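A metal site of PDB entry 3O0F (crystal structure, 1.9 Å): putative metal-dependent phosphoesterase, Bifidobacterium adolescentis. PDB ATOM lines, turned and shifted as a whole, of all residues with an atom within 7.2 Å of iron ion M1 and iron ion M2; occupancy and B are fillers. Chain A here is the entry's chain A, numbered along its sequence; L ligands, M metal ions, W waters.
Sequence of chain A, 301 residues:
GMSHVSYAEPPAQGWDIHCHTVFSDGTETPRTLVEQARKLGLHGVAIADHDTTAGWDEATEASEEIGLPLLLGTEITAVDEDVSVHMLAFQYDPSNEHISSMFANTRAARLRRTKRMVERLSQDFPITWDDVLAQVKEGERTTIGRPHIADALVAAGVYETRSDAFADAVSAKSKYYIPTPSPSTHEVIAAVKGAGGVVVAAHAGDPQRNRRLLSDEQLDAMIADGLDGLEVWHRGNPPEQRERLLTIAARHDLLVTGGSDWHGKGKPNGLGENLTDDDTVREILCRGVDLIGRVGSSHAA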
ATOM      1  N   HIS A  18     -27.400  -5.375  -2.658  1.00  0.00           N
ATOM      2  CA  HIS A  18     -27.010  -6.654  -3.234  1.00  0.00           C
ATOM      3  C   HIS A  18     -27.637  -6.838  -4.628  1.00  0.00           C
ATOM      4  O   HIS A  18     -28.668  -7.515  -4.761  1.00  0.00           O
ATOM      5  CB  HIS A  18     -27.492  -7.740  -2.292  1.00  0.00           C
ATOM      6  CG  HIS A  18     -26.834  -9.060  -2.502  1.00  0.00           C
ATOM      7  ND1 HIS A  18     -26.809 -10.040  -1.520  1.00  0.00           N
ATOM      8  CD2 HIS A  18     -26.215  -9.585  -3.586  1.00  0.00           C
ATOM      9  CE1 HIS A  18     -26.165 -11.095  -1.988  1.00  0.00           C
ATOM     10  NE2 HIS A  18     -25.799 -10.850  -3.236  1.00  0.00           N
ATOM     11  N   CYS A  19     -27.022  -6.256  -5.654  1.00  0.00           N
ATOM     12  CA  CYS A  19     -27.590  -6.227  -7.018  1.00  0.00           C
ATOM     13  C   CYS A  19     -26.490  -6.583  -8.030  1.00  0.00           C
ATOM     14  O   CYS A  19     -25.367  -6.062  -7.919  1.00  0.00           O
ATOM     15  CB  CYS A  19     -28.176  -4.870  -7.349  1.00  0.00           C
ATOM     16  SG  CYS A  19     -29.355  -4.246  -6.142  1.00  0.00           S
ATOM     17  N   HIS A  20     -26.810  -7.489  -8.960  1.00  0.00           N
ATOM     18  CA  HIS A  20     -25.912  -7.965  -9.999  1.00  0.00           C
ATOM     19  C   HIS A  20     -26.302  -7.438 -11.387  1.00  0.00           C
ATOM     20  O   HIS A  20     -27.489  -7.207 -11.647  1.00  0.00           O
ATOM     21  CB  HIS A  20     -25.918  -9.488 -10.015  1.00  0.00           C
ATOM     22  CG  HIS A  20     -25.412 -10.088  -8.747  1.00  0.00           C
ATOM     23  ND1 HIS A  20     -24.124 -10.513  -8.596  1.00  0.00           N
ATOM     24  CD2 HIS A  20     -26.025 -10.313  -7.554  1.00  0.00           C
ATOM     25  CE1 HIS A  20     -23.954 -10.971  -7.365  1.00  0.00           C
ATOM     26  NE2 HIS A  20     -25.077 -10.847  -6.718  1.00  0.00           N
ATOM     27  N   ASP A  25     -23.507 -11.933 -13.557  1.00  0.00           N
ATOM     28  CA  ASP A  25     -24.602 -12.796 -13.952  1.00  0.00           C
ATOM     29  C   ASP A  25     -26.009 -12.157 -13.979  1.00  0.00           C
ATOM     30  O   ASP A  25     -27.008 -12.867 -14.081  1.00  0.00           O
ATOM     31  CB  ASP A  25     -24.599 -14.095 -13.141  1.00  0.00           C
ATOM     32  CG  ASP A  25     -24.714 -13.894 -11.630  1.00  0.00           C
ATOM     33  OD1 ASP A  25     -24.634 -12.740 -11.112  1.00  0.00           O
ATOM     34  OD2 ASP A  25     -24.894 -14.946 -10.934  1.00  0.00           O
ATOM     35  N   ALA A  48     -22.869  -5.035  -6.866  1.00  0.00           N
ATOM     36  CA  ALA A  48     -22.157  -6.089  -6.109  1.00  0.00           C
ATOM     37  C   ALA A  48     -21.869  -7.270  -6.993  1.00  0.00           C
ATOM     38  O   ALA A  48     -22.100  -8.421  -6.595  1.00  0.00           O
ATOM     39  CB  ALA A  48     -22.983  -6.540  -4.879  1.00  0.00           C
ATOM     40  N   HIS A  50     -20.046 -10.347  -9.009  1.00  0.00           N
ATOM     41  CA  HIS A  50     -19.144 -11.429  -8.566  1.00  0.00           C
ATOM     42  C   HIS A  50     -17.706 -11.137  -8.985  1.00  0.00           C
ATOM     43  O   HIS A  50     -17.449 -10.910 -10.153  1.00  0.00           O
ATOM     44  CB  HIS A  50     -19.573 -12.747  -9.220  1.00  0.00           C
ATOM     45  CG  HIS A  50     -20.915 -13.212  -8.796  1.00  0.00           C
ATOM     46  ND1 HIS A  50     -21.123 -13.880  -7.608  1.00  0.00           N
ATOM     47  CD2 HIS A  50     -22.132 -13.106  -9.390  1.00  0.00           C
ATOM     48  CE1 HIS A  50     -22.405 -14.155  -7.482  1.00  0.00           C
ATOM     49  NE2 HIS A  50     -23.030 -13.718  -8.550  1.00  0.00           N
ATOM     50  N   GLU A  75     -19.307  -9.016  -4.846  1.00  0.00           N
ATOM     51  CA  GLU A  75     -19.604 -10.252  -4.117  1.00  0.00           C
ATOM     52  C   GLU A  75     -18.453 -11.214  -4.392  1.00  0.00           C
ATOM     53  O   GLU A  75     -18.187 -11.610  -5.522  1.00  0.00           O
ATOM     54  CB  GLU A  75     -20.956 -10.862  -4.522  1.00  0.00           C
ATOM     55  CG  GLU A  75     -21.211 -12.112  -3.761  1.00  0.00           C
ATOM     56  CD  GLU A  75     -22.646 -12.638  -3.877  1.00  0.00           C
ATOM     57  OE1 GLU A  75     -23.361 -12.176  -4.712  1.00  0.00           O
ATOM     58  OE2 GLU A  75     -23.057 -13.480  -3.037  1.00  0.00           O
ATOM     59  N   VAL A  85     -19.064 -19.851   0.701  1.00  0.00           N
ATOM     60  CA  VAL A  85     -19.415 -18.605   1.378  1.00  0.00           C
ATOM     61  C   VAL A  85     -19.245 -17.470   0.366  1.00  0.00           C
ATOM     62  O   VAL A  85     -18.210 -17.369  -0.304  1.00  0.00           O
ATOM     63  CB  VAL A  85     -18.475 -18.299   2.584  1.00  0.00           C
ATOM     64  CG1 VAL A  85     -18.896 -16.999   3.290  1.00  0.00           C
ATOM     65  CG2 VAL A  85     -18.430 -19.455   3.596  1.00  0.00           C
ATOM     66  N   HIS A  86     -20.255 -16.625   0.256  1.00  0.00           N
ATOM     67  CA  HIS A  86     -20.164 -15.416  -0.520  1.00  0.00           C
ATOM     68  C   HIS A  86     -20.040 -14.231   0.443  1.00  0.00           C
ATOM     69  O   HIS A  86     -20.783 -14.128   1.426  1.00  0.00           O
ATOM     70  CB  HIS A  86     -21.417 -15.319  -1.414  1.00  0.00           C
ATOM     71  CG  HIS A  86     -21.394 -16.282  -2.565  1.00  0.00           C
ATOM     72  ND1 HIS A  86     -22.257 -16.185  -3.644  1.00  0.00           N
ATOM     73  CD2 HIS A  86     -20.583 -17.340  -2.839  1.00  0.00           C
ATOM     74  CE1 HIS A  86     -21.991 -17.151  -4.503  1.00  0.00           C
ATOM     75  NE2 HIS A  86     -20.983 -17.860  -4.042  1.00  0.00           N
ATOM     76  N   MET A  87     -19.069 -13.364   0.146  1.00  0.00           N
ATOM     77  CA  MET A  87     -18.748 -12.208   0.977  1.00  0.00           C
ATOM     78  C   MET A  87     -19.037 -10.960   0.163  1.00  0.00           C
ATOM     79  O   MET A  87     -18.502 -10.801  -0.921  1.00  0.00           O
ATOM     80  CB  MET A  87     -17.265 -12.193   1.289  1.00  0.00           C
ATOM     81  CG  MET A  87     -16.763 -13.514   1.885  1.00  0.00           C
ATOM     82  SD  MET A  87     -16.867 -13.618   3.803  1.00  0.00           S
ATOM     83  CE  MET A  87     -17.999 -12.128   4.300  1.00  0.00           C
ATOM     84  N   LEU A  88     -19.811 -10.050   0.731  1.00  0.00           N
ATOM     85  CA  LEU A  88     -20.058  -8.752   0.118  1.00  0.00           C
ATOM     86  C   LEU A  88     -18.996  -7.785   0.672  1.00  0.00           C
ATOM     87  O   LEU A  88     -18.795  -7.724   1.887  1.00  0.00           O
ATOM     88  CB  LEU A  88     -21.471  -8.288   0.504  1.00  0.00           C
ATOM     89  CG  LEU A  88     -22.664  -9.057  -0.058  1.00  0.00           C
ATOM     90  CD1 LEU A  88     -23.921  -8.599   0.656  1.00  0.00           C
ATOM     91  CD2 LEU A  88     -22.850  -8.889  -1.560  1.00  0.00           C
ATOM     92  N   ALA A 202     -22.691 -12.840   3.118  1.00  0.00           N
ATOM     93  CA  ALA A 202     -23.930 -12.858   2.312  1.00  0.00           C
ATOM     94  C   ALA A 202     -24.782 -14.127   2.598  1.00  0.00           C
ATOM     95  O   ALA A 202     -24.233 -15.193   2.811  1.00  0.00           O
ATOM     96  CB  ALA A 202     -23.603 -12.796   0.818  1.00  0.00           C
ATOM     97  N   HIS A 203     -26.102 -13.936   2.644  1.00  0.00           N
ATOM     98  CA  HIS A 203     -27.147 -14.989   2.854  1.00  0.00           C
ATOM     99  C   HIS A 203     -26.613 -16.215   3.657  1.00  0.00           C
ATOM    100  O   HIS A 203     -26.616 -17.350   3.158  1.00  0.00           O
ATOM    101  CB  HIS A 203     -27.731 -15.407   1.480  1.00  0.00           C
ATOM    102  CG  HIS A 203     -26.695 -15.645   0.419  1.00  0.00           C
ATOM    103  ND1 HIS A 203     -25.810 -16.707   0.459  1.00  0.00           N
ATOM    104  CD2 HIS A 203     -26.388 -14.947  -0.712  1.00  0.00           C
ATOM    105  CE1 HIS A 203     -24.995 -16.655  -0.584  1.00  0.00           C
ATOM    106  NE2 HIS A 203     -25.325 -15.597  -1.308  1.00  0.00           N
ATOM    107  N   ASP A 206     -28.643 -19.637   4.253  1.00  0.00           N
ATOM    108  CA  ASP A 206     -29.309 -20.183   3.065  1.00  0.00           C
ATOM    109  C   ASP A 206     -28.863 -21.649   2.788  1.00  0.00           C
ATOM    110  O   ASP A 206     -27.716 -21.886   2.463  1.00  0.00           O
ATOM    111  CB  ASP A 206     -29.054 -19.247   1.865  1.00  0.00           C
ATOM    112  CG  ASP A 206     -29.767 -19.670   0.606  1.00  0.00           C
ATOM    113  OD1 ASP A 206     -30.487 -20.698   0.585  1.00  0.00           O
ATOM    114  OD2 ASP A 206     -29.621 -18.939  -0.401  1.00  0.00           O
ATOM    115  N   GLU A 231     -25.629 -10.293   6.359  1.00  0.00           N
ATOM    116  CA  GLU A 231     -26.796 -10.054   5.554  1.00  0.00           C
ATOM    117  C   GLU A 231     -27.897 -10.924   6.119  1.00  0.00           C
ATOM    118  O   GLU A 231     -27.814 -12.157   6.034  1.00  0.00           O
ATOM    119  CB  GLU A 231     -26.504 -10.426   4.095  1.00  0.00           C
ATOM    120  CG  GLU A 231     -27.704 -10.313   3.213  1.00  0.00           C
ATOM    121  CD  GLU A 231     -27.366 -10.553   1.748  1.00  0.00           C
ATOM    122  OE1 GLU A 231     -26.887 -11.676   1.427  1.00  0.00           O
ATOM    123  OE2 GLU A 231     -27.584  -9.639   0.918  1.00  0.00           O
ATOM    124  N   HIS A 234     -32.836 -11.312   3.513  1.00  0.00           N
ATOM    125  CA  HIS A 234     -32.552 -11.932   2.225  1.00  0.00           C
ATOM    126  C   HIS A 234     -33.508 -13.099   2.081  1.00  0.00           C
ATOM    127  O   HIS A 234     -33.758 -13.823   3.036  1.00  0.00           O
ATOM    128  CB  HIS A 234     -31.106 -12.411   2.168  1.00  0.00           C
ATOM    129  CG  HIS A 234     -30.673 -12.963   0.840  1.00  0.00           C
ATOM    130  ND1 HIS A 234     -30.990 -14.232   0.415  1.00  0.00           N
ATOM    131  CD2 HIS A 234     -29.878 -12.431  -0.132  1.00  0.00           C
ATOM    132  CE1 HIS A 234     -30.470 -14.439  -0.783  1.00  0.00           C
ATOM    133  NE2 HIS A 234     -29.775 -13.378  -1.133  1.00  0.00           N
ATOM    134  N   SER A 260     -31.695  -7.639  -2.299  1.00  0.00           N
ATOM    135  CA  SER A 260     -32.573  -8.466  -3.119  1.00  0.00           C
ATOM    136  C   SER A 260     -31.866  -9.633  -3.782  1.00  0.00           C
ATOM    137  O   SER A 260     -32.502 -10.633  -4.060  1.00  0.00           O
ATOM    138  CB  SER A 260     -33.214  -7.641  -4.207  1.00  0.00           C
ATOM    139  OG  SER A 260     -32.221  -7.080  -5.059  1.00  0.00           O
ATOM    140  N   ASP A 261     -30.550  -9.516  -4.011  1.00  0.00           N
ATOM    141  CA  ASP A 261     -29.854 -10.420  -4.912  1.00  0.00           C
ATOM    142  C   ASP A 261     -30.492 -10.360  -6.311  1.00  0.00           C
ATOM    143  O   ASP A 261     -30.597 -11.364  -6.983  1.00  0.00           O
ATOM    144  CB  ASP A 261     -29.900 -11.848  -4.381  1.00  0.00           C
ATOM    145  CG  ASP A 261     -28.574 -12.510  -4.423  1.00  0.00           C
ATOM    146  OD1 ASP A 261     -27.768 -12.117  -5.278  1.00  0.00           O
ATOM    147  OD2 ASP A 261     -28.349 -13.384  -3.570  1.00  0.00           O
ATOM    148  N   TRP A 262     -30.911  -9.176  -6.721  1.00  0.00           N
ATOM    149  CA  TRP A 262     -31.437  -8.976  -8.045  1.00  0.00           C
ATOM    150  C   TRP A 262     -30.410  -9.343  -9.096  1.00  0.00           C
ATOM    151  O   TRP A 262     -29.231  -8.954  -9.018  1.00  0.00           O
ATOM    152  CB  TRP A 262     -31.821  -7.525  -8.189  1.00  0.00           C
ATOM    153  CG  TRP A 262     -32.431  -7.051  -9.460  1.00  0.00           C
ATOM    154  CD1 TRP A 262     -33.717  -7.179  -9.830  1.00  0.00           C
ATOM    155  CD2 TRP A 262     -31.796  -6.225 -10.445  1.00  0.00           C
ATOM    156  NE1 TRP A 262     -33.936  -6.520 -11.022  1.00  0.00           N
ATOM    157  CE2 TRP A 262     -32.779  -5.879 -11.385  1.00  0.00           C
ATOM    158  CE3 TRP A 262     -30.489  -5.736 -10.606  1.00  0.00           C
ATOM    159  CZ2 TRP A 262     -32.484  -5.117 -12.498  1.00  0.00           C
ATOM    160  CZ3 TRP A 262     -30.198  -4.954 -11.706  1.00  0.00           C
ATOM    161  CH2 TRP A 262     -31.204  -4.656 -12.636  1.00  0.00           C
ATOM    162  N   HIS A 263     -30.896 -10.064 -10.100  1.00  0.00           N
ATOM    163  CA  HIS A 263     -30.128 -10.374 -11.282  1.00  0.00           C
ATOM    164  C   HIS A 263     -30.964 -10.032 -12.515  1.00  0.00           C
ATOM    165  O   HIS A 263     -30.789 -10.624 -13.586  1.00  0.00           O
ATOM    166  CB  HIS A 263     -29.809 -11.877 -11.305  1.00  0.00           C
ATOM    167  CG  HIS A 263     -28.807 -12.331 -10.297  1.00  0.00           C
ATOM    168  ND1 HIS A 263     -29.011 -12.288  -8.928  1.00  0.00           N
ATOM    169  CD2 HIS A 263     -27.590 -12.894 -10.463  1.00  0.00           C
ATOM    170  CE1 HIS A 263     -27.966 -12.792  -8.311  1.00  0.00           C
ATOM    171  NE2 HIS A 263     -27.094 -13.177  -9.223  1.00  0.00           N
ATOM    172  N   LYS A 267     -33.237 -14.129 -12.349  1.00  0.00           N
ATOM    173  CA  LYS A 267     -33.802 -14.736 -11.162  1.00  0.00           C
ATOM    174  C   LYS A 267     -35.164 -14.116 -10.912  1.00  0.00           C
ATOM    175  O   LYS A 267     -35.448 -13.052 -11.399  1.00  0.00           O
ATOM    176  CB  LYS A 267     -32.904 -14.456  -9.940  1.00  0.00           C
ATOM    177  CG  LYS A 267     -31.667 -15.327  -9.762  1.00  0.00           C
ATOM    178  CD  LYS A 267     -31.074 -15.075  -8.385  1.00  0.00           C
ATOM    179  CE  LYS A 267     -29.792 -15.831  -8.092  1.00  0.00           C
ATOM    180  NZ  LYS A 267     -29.399 -15.511  -6.692  1.00  0.00           N
HETATM  181  P1  LIG L   1     -25.693 -15.163  -6.479  1.00  0.00           P
HETATM  182  O1  LIG L   1     -27.040 -15.807  -6.203  1.00  0.00           O
HETATM  183  O2  LIG L   1     -24.689 -15.830  -5.564  1.00  0.00           O
HETATM  184  O3  LIG L   1     -25.348 -15.108  -7.987  1.00  0.00           O
HETATM  185  O4  LIG L   1     -25.703 -13.701  -6.220  1.00  0.00           O
HETATM  186  P1  LG2 L   2     -20.994 -20.536  -9.932  1.00  0.00           P
HETATM  187  O1  LG2 L   2     -20.421 -19.565  -8.950  1.00  0.00           O
HETATM  188  O2  LG2 L   2     -20.362 -20.321 -11.283  1.00  0.00           O
HETATM  189  O3  LG2 L   2     -20.996 -21.992  -9.462  1.00  0.00           O
HETATM  190  O4  LG2 L   2     -22.534 -20.128 -10.110  1.00  0.00           O
HETATM  191  C1  LG2 L   2     -23.440 -20.287  -9.041  1.00  0.00           C
HETATM  192  C2  LG2 L   2     -24.188 -18.996  -8.909  1.00  0.00           C
HETATM  193  O5  LG2 L   2     -25.227 -18.853  -9.910  1.00  0.00           O
HETATM  194  C3  LG2 L   2     -24.851 -18.895  -7.542  1.00  0.00           C
HETATM  195  O6  LG2 L   2     -24.142 -17.950  -6.751  1.00  0.00           O
HETATM  196  C4  LG2 L   2     -26.194 -18.329  -7.965  1.00  0.00           C
HETATM  197  O7  LG2 L   2     -27.235 -17.963  -7.065  1.00  0.00           O
HETATM  198  C5  LG2 L   2     -26.084 -17.837  -9.408  1.00  0.00           C
HETATM  199  N1  LG2 L   2     -27.393 -17.759 -10.090  1.00  0.00           N
HETATM  200  C6  LG2 L   2     -27.756 -16.782 -10.918  1.00  0.00           C
HETATM  201  N2  LG2 L   2     -29.004 -17.012 -11.386  1.00  0.00           N
HETATM  202  C7  LG2 L   2     -29.452 -18.154 -10.845  1.00  0.00           C
HETATM  203  C8  LG2 L   2     -30.689 -18.952 -10.911  1.00  0.00           C
HETATM  204  N3  LG2 L   2     -31.752 -18.554 -11.689  1.00  0.00           N
HETATM  205  N4  LG2 L   2     -30.714 -20.090 -10.202  1.00  0.00           N
HETATM  206  C9  LG2 L   2     -29.691 -20.520  -9.430  1.00  0.00           C
HETATM  207  N5  LG2 L   2     -28.548 -19.838  -9.317  1.00  0.00           N
HETATM  208  C10 LG2 L   2     -28.382 -18.659  -9.987  1.00  0.00           C
HETATM  209 FE    FE M   1     -25.510 -12.234  -4.937  1.00  0.00          FE
HETATM  210 FE    FE M   2     -24.414 -15.109  -3.357  1.00  0.00          FE
HETATM  211 ZN    ZN M   3     -25.098 -13.733  -9.051  1.00  0.00          ZN
HETATM  212  O   HOH W   1     -25.862 -13.727  -3.528  1.00  0.00           O
HETATM  213  O   HOH W   2     -26.853 -17.438  -3.722  1.00  0.00           O
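An oxygen (O7) of LG2 L2 lies within hydrogen-bond range of the side-chain amino group (NZ) of Lys 267 (3.3 Å).
Iron ion M2 is bound by water W1 (2.0 Å), the side-chain carboxylate (OE2) of Glu 75 (2.1 Å), a ring nitrogen (NE2) of His 203 (2.3 Å), an oxygen (O2) of LIG L1 (2.3 Å) and a ring nitrogen (ND1) of His 86 (2.4 Å). Iron ion M2 has five donor atoms within binding distance.
Iron ion M1 is bound by an oxygen (O4) of LIG L1, water W1, the side-chain carboxylate (OE1) of Glu 75, a ring nitrogen (NE2) of His 18, the side-chain carboxylate (OD1) of Asp 261 and a ring nitrogen (NE2) of His 20.
O of His 86 lies within hydrogen-bond range of N of Ala 202. OD1 of Asp 25 lies close to ND1 of His 20, at 3.4 Å. A ring nitrogen (ND1) of His 20 lies close to a ring nitrogen (NE2) of His 50 (3.4 Å). OD2 of Asp 261 lies within salt-bridge range of NZ of Lys 267 (3.9 Å). O of His 18 sits at hydrogen-bond distance from N of Trp 262 (3.4 Å). A ring nitrogen (ND1) of His 18 sits at hydrogen-bond distance from the side-chain carboxylate of Glu 231, at 2.6 Å. ND1 of His 263 lies within hydrogen-bond range of O of Asp 261. The backbone NH (N) of His 20 lies within hydrogen-bond range of the backbone carbonyl oxygen (O) of Trp 262, 2.8 Å away.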
